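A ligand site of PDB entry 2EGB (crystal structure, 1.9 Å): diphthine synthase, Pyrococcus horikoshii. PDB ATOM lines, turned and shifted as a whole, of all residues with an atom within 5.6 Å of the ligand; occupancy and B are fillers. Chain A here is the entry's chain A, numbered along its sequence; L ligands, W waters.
A nitrogen (N1) of the ligand sits at hydrogen-bond distance from the backbone carbonyl oxygen (O) of Val 90 (2.6 Å).
O of His 234 sits at hydrogen-bond distance from O5 of the ligand (2.6 Å).
The backbone NH of Leu 166 lies within hydrogen-bond range of an oxygen (O5) of the ligand.
The backbone carbonyl oxygen (O) of Leu 166 is in hydrogen-bond range of an oxygen (O4) of the ligand, 2.7 Å away.
O1 of the ligand sits at hydrogen-bond distance from OG of Ser 115, 2.8 Å away.
N5 of the ligand is in hydrogen-bond range of N of Ala 209 (3.0 Å).
O of Ala 209 lies within hydrogen-bond range of N4 of the ligand (2.8 Å).
The backbone NH (N) of Asp 87 is in hydrogen-bond range of an oxygen (O1) of the ligand (2.8 Å).
The backbone carbonyl oxygen (O) of Asp 87 is in hydrogen-bond range of a nitrogen (N1) of the ligand (2.8 Å).
O2 of the ligand is in hydrogen-bond range of N of Ile 116.
O of Leu 10 sits at hydrogen-bond distance from N4 of the ligand.
OG of Ser 37 sits close to N3 of the ligand (3.5 Å).
The backbone NH (N) of Tyr 117 lies close to the side-chain hydroxyl (OG) of Ser 115 (3.2 Å).
The side-chain carboxylate (OD1) of Asp 87 sits at hydrogen-bond distance from the backbone NH (N) of Leu 89 (3.0 Å).
The backbone NH (N) of Arg 208 is in hydrogen-bond range of the backbone carbonyl oxygen (O) of Pro 233.
N of Ile 235 lies within hydrogen-bond range of O of Leu 206 (3.0 Å).
The side-chain hydroxyl of Thr 92 is in hydrogen-bond range of the backbone carbonyl oxygen of Pro 88, at 2.8 Å.
The backbone carbonyl oxygen of Thr 36 lies close to a sulfur (S1) of the ligand, at 3.7 Å.
Pro 85 touches the ligand (O to N1, 3.97 Å).
CA of Gly 86 touches C4 of the ligand, at 3.7 Å.
Ala 91 touches the ligand.
Thr 92 touches the ligand.
Phe 165 touches the ligand.
Leu 206 touches the ligand (O to C13, 3.6 Å).
Arg 208 touches the ligand.
Pro 233 touches the ligand (O to C13, 3.5 Å).
CB of Ile 235 touches N6 of the ligand, at 3.7 Å.
Hydrophobic or aromatic side chains that line the ligand: Leu 10, Val 90, Ala 91, Ile 116, Phe 165, Leu 166, Ala 209, Pro 233 and Ile 235.
The nearest printed residue that does not touch the ligand is Asp 167 (4.3 Å).
Water W2 lies within hydrogen-bond range of O4 of the ligand (2.8 Å) and O of Asp 167 (3.0 Å).
Water W3 lies within hydrogen-bond range of OG1 of Thr 36 (2.7 Å), N1 of the ligand (2.8 Å) and O of Pro 85 (3.0 Å).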
ATOM      1  N   LEU A  10       2.404  18.237   6.109  1.00  0.00           N
ATOM      2  CA  LEU A  10       2.013  19.418   6.888  1.00  0.00           C
ATOM      3  C   LEU A  10       0.784  20.272   6.597  1.00  0.00           C
ATOM      4  O   LEU A  10       0.076  20.647   7.530  1.00  0.00           O
ATOM      5  CB  LEU A  10       3.200  20.375   6.925  1.00  0.00           C
ATOM      6  CG  LEU A  10       4.543  19.847   7.419  1.00  0.00           C
ATOM      7  CD1 LEU A  10       5.655  20.773   6.966  1.00  0.00           C
ATOM      8  CD2 LEU A  10       4.519  19.702   8.925  1.00  0.00           C
ATOM      9  N   TYR A  11       0.531  20.577   5.331  1.00  0.00           N
ATOM     10  CA  TYR A  11      -0.548  21.510   5.012  1.00  0.00           C
ATOM     11  C   TYR A  11      -1.561  21.111   3.945  1.00  0.00           C
ATOM     12  O   TYR A  11      -2.764  21.209   4.172  1.00  0.00           O
ATOM     13  CB  TYR A  11       0.131  22.835   4.617  1.00  0.00           C
ATOM     14  CG  TYR A  11      -0.780  24.006   4.315  1.00  0.00           C
ATOM     15  CD1 TYR A  11      -1.514  24.624   5.329  1.00  0.00           C
ATOM     16  CD2 TYR A  11      -0.876  24.510   3.025  1.00  0.00           C
ATOM     17  CE1 TYR A  11      -2.313  25.738   5.055  1.00  0.00           C
ATOM     18  CE2 TYR A  11      -1.677  25.625   2.741  1.00  0.00           C
ATOM     19  CZ  TYR A  11      -2.392  26.228   3.760  1.00  0.00           C
ATOM     20  OH  TYR A  11      -3.188  27.312   3.484  1.00  0.00           O
ATOM     21  N   THR A  36      -5.545  13.488  14.438  1.00  0.00           N
ATOM     22  CA  THR A  36      -4.260  13.715  15.109  1.00  0.00           C
ATOM     23  C   THR A  36      -3.660  15.070  14.789  1.00  0.00           C
ATOM     24  O   THR A  36      -2.829  15.587  15.538  1.00  0.00           O
ATOM     25  CB  THR A  36      -3.226  12.618  14.746  1.00  0.00           C
ATOM     26  OG1 THR A  36      -3.052  12.575  13.324  1.00  0.00           O
ATOM     27  CG2 THR A  36      -3.692  11.265  15.237  1.00  0.00           C
ATOM     28  N   SER A  37      -4.078  15.662  13.676  1.00  0.00           N
ATOM     29  CA  SER A  37      -3.569  16.975  13.296  1.00  0.00           C
ATOM     30  C   SER A  37      -4.528  17.612  12.306  1.00  0.00           C
ATOM     31  O   SER A  37      -5.526  16.995  11.910  1.00  0.00           O
ATOM     32  CB  SER A  37      -2.178  16.848  12.673  1.00  0.00           C
ATOM     33  OG  SER A  37      -1.620  18.122  12.454  1.00  0.00           O
ATOM     34  N   LEU A  38      -4.216  18.837  11.904  1.00  0.00           N
ATOM     35  CA  LEU A  38      -5.048  19.558  10.955  1.00  0.00           C
ATOM     36  C   LEU A  38      -4.285  19.988   9.703  1.00  0.00           C
ATOM     37  O   LEU A  38      -3.249  20.653   9.789  1.00  0.00           O
ATOM     38  CB  LEU A  38      -5.649  20.807  11.620  1.00  0.00           C
ATOM     39  CG  LEU A  38      -6.451  21.748  10.705  1.00  0.00           C
ATOM     40  CD1 LEU A  38      -7.748  21.056  10.295  1.00  0.00           C
ATOM     41  CD2 LEU A  38      -6.754  23.061  11.424  1.00  0.00           C
ATOM     42  N   PRO A  85      -2.157  12.837   8.731  1.00  0.00           N
ATOM     43  CA  PRO A  85      -1.531  14.125   8.442  1.00  0.00           C
ATOM     44  C   PRO A  85      -0.066  14.019   8.901  1.00  0.00           C
ATOM     45  O   PRO A  85       0.273  13.111   9.667  1.00  0.00           O
ATOM     46  CB  PRO A  85      -2.318  15.101   9.312  1.00  0.00           C
ATOM     47  CG  PRO A  85      -3.666  14.440   9.438  1.00  0.00           C
ATOM     48  CD  PRO A  85      -3.307  12.995   9.642  1.00  0.00           C
ATOM     49  N   GLY A  86       0.781  14.934   8.428  1.00  0.00           N
ATOM     50  CA  GLY A  86       2.190  14.922   8.804  1.00  0.00           C
ATOM     51  C   GLY A  86       2.831  13.560   8.663  1.00  0.00           C
ATOM     52  O   GLY A  86       2.604  12.877   7.664  1.00  0.00           O
ATOM     53  N   ASP A  87       3.662  13.177   9.628  1.00  0.00           N
ATOM     54  CA  ASP A  87       4.312  11.867   9.622  1.00  0.00           C
ATOM     55  C   ASP A  87       3.436  10.986  10.521  1.00  0.00           C
ATOM     56  O   ASP A  87       3.114  11.356  11.647  1.00  0.00           O
ATOM     57  CB  ASP A  87       5.729  11.959  10.198  1.00  0.00           C
ATOM     58  CG  ASP A  87       6.479  10.635  10.143  1.00  0.00           C
ATOM     59  OD1 ASP A  87       6.097   9.708  10.870  1.00  0.00           O
ATOM     60  OD2 ASP A  87       7.446  10.541   9.359  1.00  0.00           O
ATOM     61  N   PRO A  88       3.035   9.808  10.025  1.00  0.00           N
ATOM     62  CA  PRO A  88       2.180   8.889  10.770  1.00  0.00           C
ATOM     63  C   PRO A  88       2.616   8.431  12.164  1.00  0.00           C
ATOM     64  O   PRO A  88       1.777   8.074  12.984  1.00  0.00           O
ATOM     65  CB  PRO A  88       2.006   7.712   9.805  1.00  0.00           C
ATOM     66  CG  PRO A  88       3.289   7.721   9.032  1.00  0.00           C
ATOM     67  CD  PRO A  88       3.518   9.193   8.769  1.00  0.00           C
ATOM     68  N   LEU A  89       3.919   8.462  12.436  1.00  0.00           N
ATOM     69  CA  LEU A  89       4.413   8.009  13.731  1.00  0.00           C
ATOM     70  C   LEU A  89       4.977   9.105  14.635  1.00  0.00           C
ATOM     71  O   LEU A  89       5.655   8.810  15.627  1.00  0.00           O
ATOM     72  CB  LEU A  89       5.487   6.946  13.515  1.00  0.00           C
ATOM     73  CG  LEU A  89       5.112   5.746  12.647  1.00  0.00           C
ATOM     74  CD1 LEU A  89       6.252   4.733  12.654  1.00  0.00           C
ATOM     75  CD2 LEU A  89       3.838   5.094  13.168  1.00  0.00           C
ATOM     76  N   VAL A  90       4.692  10.367  14.318  1.00  0.00           N
ATOM     77  CA  VAL A  90       5.180  11.468  15.140  1.00  0.00           C
ATOM     78  C   VAL A  90       4.058  12.080  15.961  1.00  0.00           C
ATOM     79  O   VAL A  90       3.061  12.548  15.420  1.00  0.00           O
ATOM     80  CB  VAL A  90       5.800  12.583  14.272  1.00  0.00           C
ATOM     81  CG1 VAL A  90       6.177  13.773  15.150  1.00  0.00           C
ATOM     82  CG2 VAL A  90       7.042  12.059  13.568  1.00  0.00           C
ATOM     83  N   ALA A  91       4.225  12.063  17.285  1.00  0.00           N
ATOM     84  CA  ALA A  91       3.226  12.647  18.185  1.00  0.00           C
ATOM     85  C   ALA A  91       1.846  12.019  17.989  1.00  0.00           C
ATOM     86  O   ALA A  91       0.829  12.707  18.046  1.00  0.00           O
ATOM     87  CB  ALA A  91       3.150  14.161  17.978  1.00  0.00           C
ATOM     88  N   THR A  92       1.851  10.721  17.738  1.00  0.00           N
ATOM     89  CA  THR A  92       0.622   9.956  17.586  1.00  0.00           C
ATOM     90  C   THR A  92       0.958   8.657  18.292  1.00  0.00           C
ATOM     91  O   THR A  92       2.104   8.440  18.700  1.00  0.00           O
ATOM     92  CB  THR A  92       0.293   9.608  16.113  1.00  0.00           C
ATOM     93  OG1 THR A  92       1.202   8.619  15.634  1.00  0.00           O
ATOM     94  CG2 THR A  92       0.376  10.857  15.235  1.00  0.00           C
ATOM     95  N   PRO A 114       6.670  15.166   5.538  1.00  0.00           N
ATOM     96  CA  PRO A 114       7.120  16.296   6.351  1.00  0.00           C
ATOM     97  C   PRO A 114       6.353  16.342   7.679  1.00  0.00           C
ATOM     98  O   PRO A 114       5.134  16.162   7.709  1.00  0.00           O
ATOM     99  CB  PRO A 114       6.812  17.514   5.477  1.00  0.00           C
ATOM    100  CG  PRO A 114       6.849  16.949   4.078  1.00  0.00           C
ATOM    101  CD  PRO A 114       6.199  15.613   4.215  1.00  0.00           C
ATOM    102  N   SER A 115       7.085  16.570   8.764  1.00  0.00           N
ATOM    103  CA  SER A 115       6.502  16.613  10.103  1.00  0.00           C
ATOM    104  C   SER A 115       6.759  17.961  10.773  1.00  0.00           C
ATOM    105  O   SER A 115       7.795  18.590  10.555  1.00  0.00           O
ATOM    106  CB  SER A 115       7.123  15.509  10.968  1.00  0.00           C
ATOM    107  OG  SER A 115       6.695  15.609  12.319  1.00  0.00           O
ATOM    108  N   ILE A 116       5.822  18.407  11.596  1.00  0.00           N
ATOM    109  CA  ILE A 116       5.990  19.683  12.276  1.00  0.00           C
ATOM    110  C   ILE A 116       7.213  19.610  13.199  1.00  0.00           C
ATOM    111  O   ILE A 116       7.863  20.613  13.482  1.00  0.00           O
ATOM    112  CB  ILE A 116       4.739  20.048  13.111  1.00  0.00           C
ATOM    113  CG1 ILE A 116       4.885  21.470  13.669  1.00  0.00           C
ATOM    114  CG2 ILE A 116       4.558  19.051  14.256  1.00  0.00           C
ATOM    115  CD1 ILE A 116       4.935  22.550  12.595  1.00  0.00           C
ATOM    116  N   TYR A 117       7.512  18.398  13.670  1.00  0.00           N
ATOM    117  CA  TYR A 117       8.644  18.192  14.571  1.00  0.00           C
ATOM    118  C   TYR A 117       9.963  18.657  13.955  1.00  0.00           C
ATOM    119  O   TYR A 117      10.835  19.175  14.662  1.00  0.00           O
ATOM    120  CB  TYR A 117       8.702  16.706  14.950  1.00  0.00           C
ATOM    121  CG  TYR A 117       9.777  16.351  15.963  1.00  0.00           C
ATOM    122  CD1 TYR A 117       9.752  16.860  17.263  1.00  0.00           C
ATOM    123  CD2 TYR A 117      10.791  15.463  15.617  1.00  0.00           C
ATOM    124  CE1 TYR A 117      10.714  16.478  18.202  1.00  0.00           C
ATOM    125  CE2 TYR A 117      11.760  15.080  16.544  1.00  0.00           C
ATOM    126  CZ  TYR A 117      11.718  15.582  17.827  1.00  0.00           C
ATOM    127  OH  TYR A 117      12.676  15.190  18.725  1.00  0.00           O
ATOM    128  N   LEU A 164       6.205  23.010  21.700  1.00  0.00           N
ATOM    129  CA  LEU A 164       4.930  22.740  22.345  1.00  0.00           C
ATOM    130  C   LEU A 164       3.844  22.472  21.325  1.00  0.00           C
ATOM    131  O   LEU A 164       3.380  23.390  20.637  1.00  0.00           O
ATOM    132  CB  LEU A 164       4.516  23.928  23.225  1.00  0.00           C
ATOM    133  CG  LEU A 164       5.427  24.250  24.410  1.00  0.00           C
ATOM    134  CD1 LEU A 164       5.090  25.630  24.955  1.00  0.00           C
ATOM    135  CD2 LEU A 164       5.267  23.186  25.494  1.00  0.00           C
ATOM    136  N   PHE A 165       3.466  21.203  21.203  1.00  0.00           N
ATOM    137  CA  PHE A 165       2.397  20.809  20.308  1.00  0.00           C
ATOM    138  C   PHE A 165       1.153  21.386  20.995  1.00  0.00           C
ATOM    139  O   PHE A 165       1.095  21.399  22.218  1.00  0.00           O
ATOM    140  CB  PHE A 165       2.282  19.275  20.276  1.00  0.00           C
ATOM    141  CG  PHE A 165       3.464  18.581  19.653  1.00  0.00           C
ATOM    142  CD1 PHE A 165       3.551  18.436  18.270  1.00  0.00           C
ATOM    143  CD2 PHE A 165       4.481  18.071  20.446  1.00  0.00           C
ATOM    144  CE1 PHE A 165       4.634  17.775  17.686  1.00  0.00           C
ATOM    145  CE2 PHE A 165       5.577  17.407  19.869  1.00  0.00           C
ATOM    146  CZ  PHE A 165       5.645  17.266  18.492  1.00  0.00           C
ATOM    147  N   LEU A 166       0.186  21.864  20.218  1.00  0.00           N
ATOM    148  CA  LEU A 166      -1.027  22.432  20.802  1.00  0.00           C
ATOM    149  C   LEU A 166      -2.197  21.468  20.646  1.00  0.00           C
ATOM    150  O   LEU A 166      -2.284  20.723  19.667  1.00  0.00           O
ATOM    151  CB  LEU A 166      -1.331  23.785  20.162  1.00  0.00           C
ATOM    152  CG  LEU A 166      -0.178  24.803  20.254  1.00  0.00           C
ATOM    153  CD1 LEU A 166      -0.642  26.155  19.763  1.00  0.00           C
ATOM    154  CD2 LEU A 166       0.320  24.906  21.699  1.00  0.00           C
ATOM    155  N   ASP A 167      -3.118  21.492  21.610  1.00  0.00           N
ATOM    156  CA  ASP A 167      -4.239  20.560  21.598  1.00  0.00           C
ATOM    157  C   ASP A 167      -5.181  20.666  20.400  1.00  0.00           C
ATOM    158  O   ASP A 167      -5.236  21.694  19.707  1.00  0.00           O
ATOM    159  CB  ASP A 167      -5.051  20.697  22.881  1.00  0.00           C
ATOM    160  CG  ASP A 167      -5.735  19.404  23.269  1.00  0.00           C
ATOM    161  OD1 ASP A 167      -5.681  18.434  22.479  1.00  0.00           O
ATOM    162  OD2 ASP A 167      -6.315  19.341  24.374  1.00  0.00           O
ATOM    163  N   ILE A 168      -5.902  19.587  20.155  1.00  0.00           N
ATOM    164  CA  ILE A 168      -6.849  19.512  19.054  1.00  0.00           C
ATOM    165  C   ILE A 168      -8.007  18.595  19.416  1.00  0.00           C
ATOM    166  O   ILE A 168      -7.815  17.534  20.018  1.00  0.00           O
ATOM    167  CB  ILE A 168      -6.172  18.985  17.769  1.00  0.00           C
ATOM    168  CG1 ILE A 168      -7.217  18.829  16.650  1.00  0.00           C
ATOM    169  CG2 ILE A 168      -5.489  17.651  18.043  1.00  0.00           C
ATOM    170  CD1 ILE A 168      -6.644  18.367  15.324  1.00  0.00           C
ATOM    171  N   LEU A 206       4.715  29.407  15.119  1.00  0.00           N
ATOM    172  CA  LEU A 206       4.775  28.950  13.750  1.00  0.00           C
ATOM    173  C   LEU A 206       3.372  28.489  13.413  1.00  0.00           C
ATOM    174  O   LEU A 206       2.853  27.552  14.042  1.00  0.00           O
ATOM    175  CB  LEU A 206       5.755  27.776  13.596  1.00  0.00           C
ATOM    176  CG  LEU A 206       5.840  27.149  12.191  1.00  0.00           C
ATOM    177  CD1 LEU A 206       6.155  28.229  11.147  1.00  0.00           C
ATOM    178  CD2 LEU A 206       6.921  26.077  12.191  1.00  0.00           C
ATOM    179  N   ALA A 207       2.748  29.152  12.455  1.00  0.00           N
ATOM    180  CA  ALA A 207       1.390  28.803  12.069  1.00  0.00           C
ATOM    181  C   ALA A 207       1.334  28.362  10.618  1.00  0.00           C
ATOM    182  O   ALA A 207       1.913  29.004   9.739  1.00  0.00           O
ATOM    183  CB  ALA A 207       0.463  29.997  12.282  1.00  0.00           C
ATOM    184  N   ARG A 208       0.639  27.246  10.384  1.00  0.00           N
ATOM    185  CA  ARG A 208       0.454  26.692   9.058  1.00  0.00           C
ATOM    186  C   ARG A 208       1.746  26.371   8.328  1.00  0.00           C
ATOM    187  O   ARG A 208       1.958  26.786   7.177  1.00  0.00           O
ATOM    188  CB  ARG A 208      -0.430  27.633   8.228  1.00  0.00           C
ATOM    189  CG  ARG A 208      -1.776  27.935   8.899  1.00  0.00           C
ATOM    190  CD  ARG A 208      -2.592  28.953   8.095  1.00  0.00           C
ATOM    191  NE  ARG A 208      -1.779  30.135   7.800  1.00  0.00           N
ATOM    192  CZ  ARG A 208      -1.439  31.057   8.696  1.00  0.00           C
ATOM    193  NH1 ARG A 208      -1.844  30.955   9.958  1.00  0.00           N
ATOM    194  NH2 ARG A 208      -0.655  32.060   8.339  1.00  0.00           N
ATOM    195  N   ALA A 209       2.625  25.644   9.004  1.00  0.00           N
ATOM    196  CA  ALA A 209       3.880  25.231   8.405  1.00  0.00           C
ATOM    197  C   ALA A 209       3.470  24.352   7.230  1.00  0.00           C
ATOM    198  O   ALA A 209       2.457  23.664   7.281  1.00  0.00           O
ATOM    199  CB  ALA A 209       4.696  24.422   9.406  1.00  0.00           C
ATOM    200  N   GLY A 210       4.254  24.379   6.160  1.00  0.00           N
ATOM    201  CA  GLY A 210       3.921  23.596   4.988  1.00  0.00           C
ATOM    202  C   GLY A 210       3.366  24.487   3.897  1.00  0.00           C
ATOM    203  O   GLY A 210       3.595  24.250   2.710  1.00  0.00           O
ATOM    204  N   PRO A 233      -3.428  25.122  11.895  1.00  0.00           N
ATOM    205  CA  PRO A 233      -2.867  24.798  13.209  1.00  0.00           C
ATOM    206  C   PRO A 233      -1.710  25.706  13.585  1.00  0.00           C
ATOM    207  O   PRO A 233      -1.080  26.316  12.721  1.00  0.00           O
ATOM    208  CB  PRO A 233      -2.415  23.356  13.034  1.00  0.00           C
ATOM    209  CG  PRO A 233      -1.918  23.361  11.617  1.00  0.00           C
ATOM    210  CD  PRO A 233      -2.981  24.150  10.881  1.00  0.00           C
ATOM    211  N   HIS A 234      -1.453  25.791  14.879  1.00  0.00           N
ATOM    212  CA  HIS A 234      -0.368  26.616  15.406  1.00  0.00           C
ATOM    213  C   HIS A 234       0.496  25.743  16.296  1.00  0.00           C
ATOM    214  O   HIS A 234       0.047  24.715  16.798  1.00  0.00           O
ATOM    215  CB  HIS A 234      -0.896  27.738  16.314  1.00  0.00           C
ATOM    216  CG  HIS A 234      -1.705  28.777  15.624  1.00  0.00           C
ATOM    217  ND1 HIS A 234      -2.213  29.881  16.287  1.00  0.00           N
ATOM    218  CD2 HIS A 234      -2.101  28.909  14.337  1.00  0.00           C
ATOM    219  CE1 HIS A 234      -2.876  30.647  15.438  1.00  0.00           C
ATOM    220  NE2 HIS A 234      -2.824  30.081  14.243  1.00  0.00           N
ATOM    221  N   ILE A 235       1.735  26.167  16.501  1.00  0.00           N
ATOM    222  CA  ILE A 235       2.621  25.464  17.405  1.00  0.00           C
ATOM    223  C   ILE A 235       3.372  26.584  18.122  1.00  0.00           C
ATOM    224  O   ILE A 235       3.629  27.634  17.530  1.00  0.00           O
ATOM    225  CB  ILE A 235       3.587  24.509  16.652  1.00  0.00           C
ATOM    226  CG1 ILE A 235       4.068  23.428  17.609  1.00  0.00           C
ATOM    227  CG2 ILE A 235       4.764  25.284  16.070  1.00  0.00           C
ATOM    228  CD1 ILE A 235       4.384  22.112  16.937  1.00  0.00           C
HETATM  229  N1  LIG L   1       2.103  13.483  13.165  1.00  0.00           N
HETATM  230  C1  LIG L   1       1.938  14.998  13.056  1.00  0.00           C
HETATM  231  C2  LIG L   1       1.721  15.757  14.338  1.00  0.00           C
HETATM  232  C3  LIG L   1       0.548  15.386  15.230  1.00  0.00           C
HETATM  233  S1  LIG L   1       0.521  16.595  16.616  1.00  0.00           S
HETATM  234  C4  LIG L   1       3.226  15.550  12.297  1.00  0.00           C
HETATM  235  O1  LIG L   1       4.109  14.734  11.959  1.00  0.00           O
HETATM  236  O2  LIG L   1       3.262  16.831  12.079  1.00  0.00           O
HETATM  237  C5  LIG L   1      -0.580  17.784  15.941  1.00  0.00           C
HETATM  238  C6  LIG L   1      -0.192  19.232  16.465  1.00  0.00           C
HETATM  239  O3  LIG L   1       1.092  19.572  15.904  1.00  0.00           O
HETATM  240  C7  LIG L   1      -1.129  20.315  16.072  1.00  0.00           C
HETATM  241  O4  LIG L   1      -2.184  20.431  17.016  1.00  0.00           O
HETATM  242  C8  LIG L   1      -0.179  21.531  16.000  1.00  0.00           C
HETATM  243  O5  LIG L   1       0.042  22.117  17.277  1.00  0.00           O
HETATM  244  C9  LIG L   1       1.090  20.970  15.349  1.00  0.00           C
HETATM  245  N2  LIG L   1       1.071  20.963  14.003  1.00  0.00           N
HETATM  246  C10 LIG L   1       0.869  19.988  13.035  1.00  0.00           C
HETATM  247  N3  LIG L   1       0.944  20.413  11.808  1.00  0.00           N
HETATM  248  C11 LIG L   1       1.231  21.795  11.930  1.00  0.00           C
HETATM  249  C12 LIG L   1       1.440  22.819  10.934  1.00  0.00           C
HETATM  250  N4  LIG L   1       1.391  22.604   9.617  1.00  0.00           N
HETATM  251  N5  LIG L   1       1.704  24.080  11.441  1.00  0.00           N
HETATM  252  C13 LIG L   1       1.772  24.353  12.776  1.00  0.00           C
HETATM  253  N6  LIG L   1       1.573  23.399  13.752  1.00  0.00           N
HETATM  254  C14 LIG L   1       1.314  22.147  13.254  1.00  0.00           C
HETATM  255  O   HOH W   1       1.353  17.953  10.328  1.00  0.00           O
HETATM  256  O   HOH W   2      -4.313  22.206  16.917  1.00  0.00           O
HETATM  257  O   HOH W   3      -0.603  13.216  12.484  1.00  0.00           O
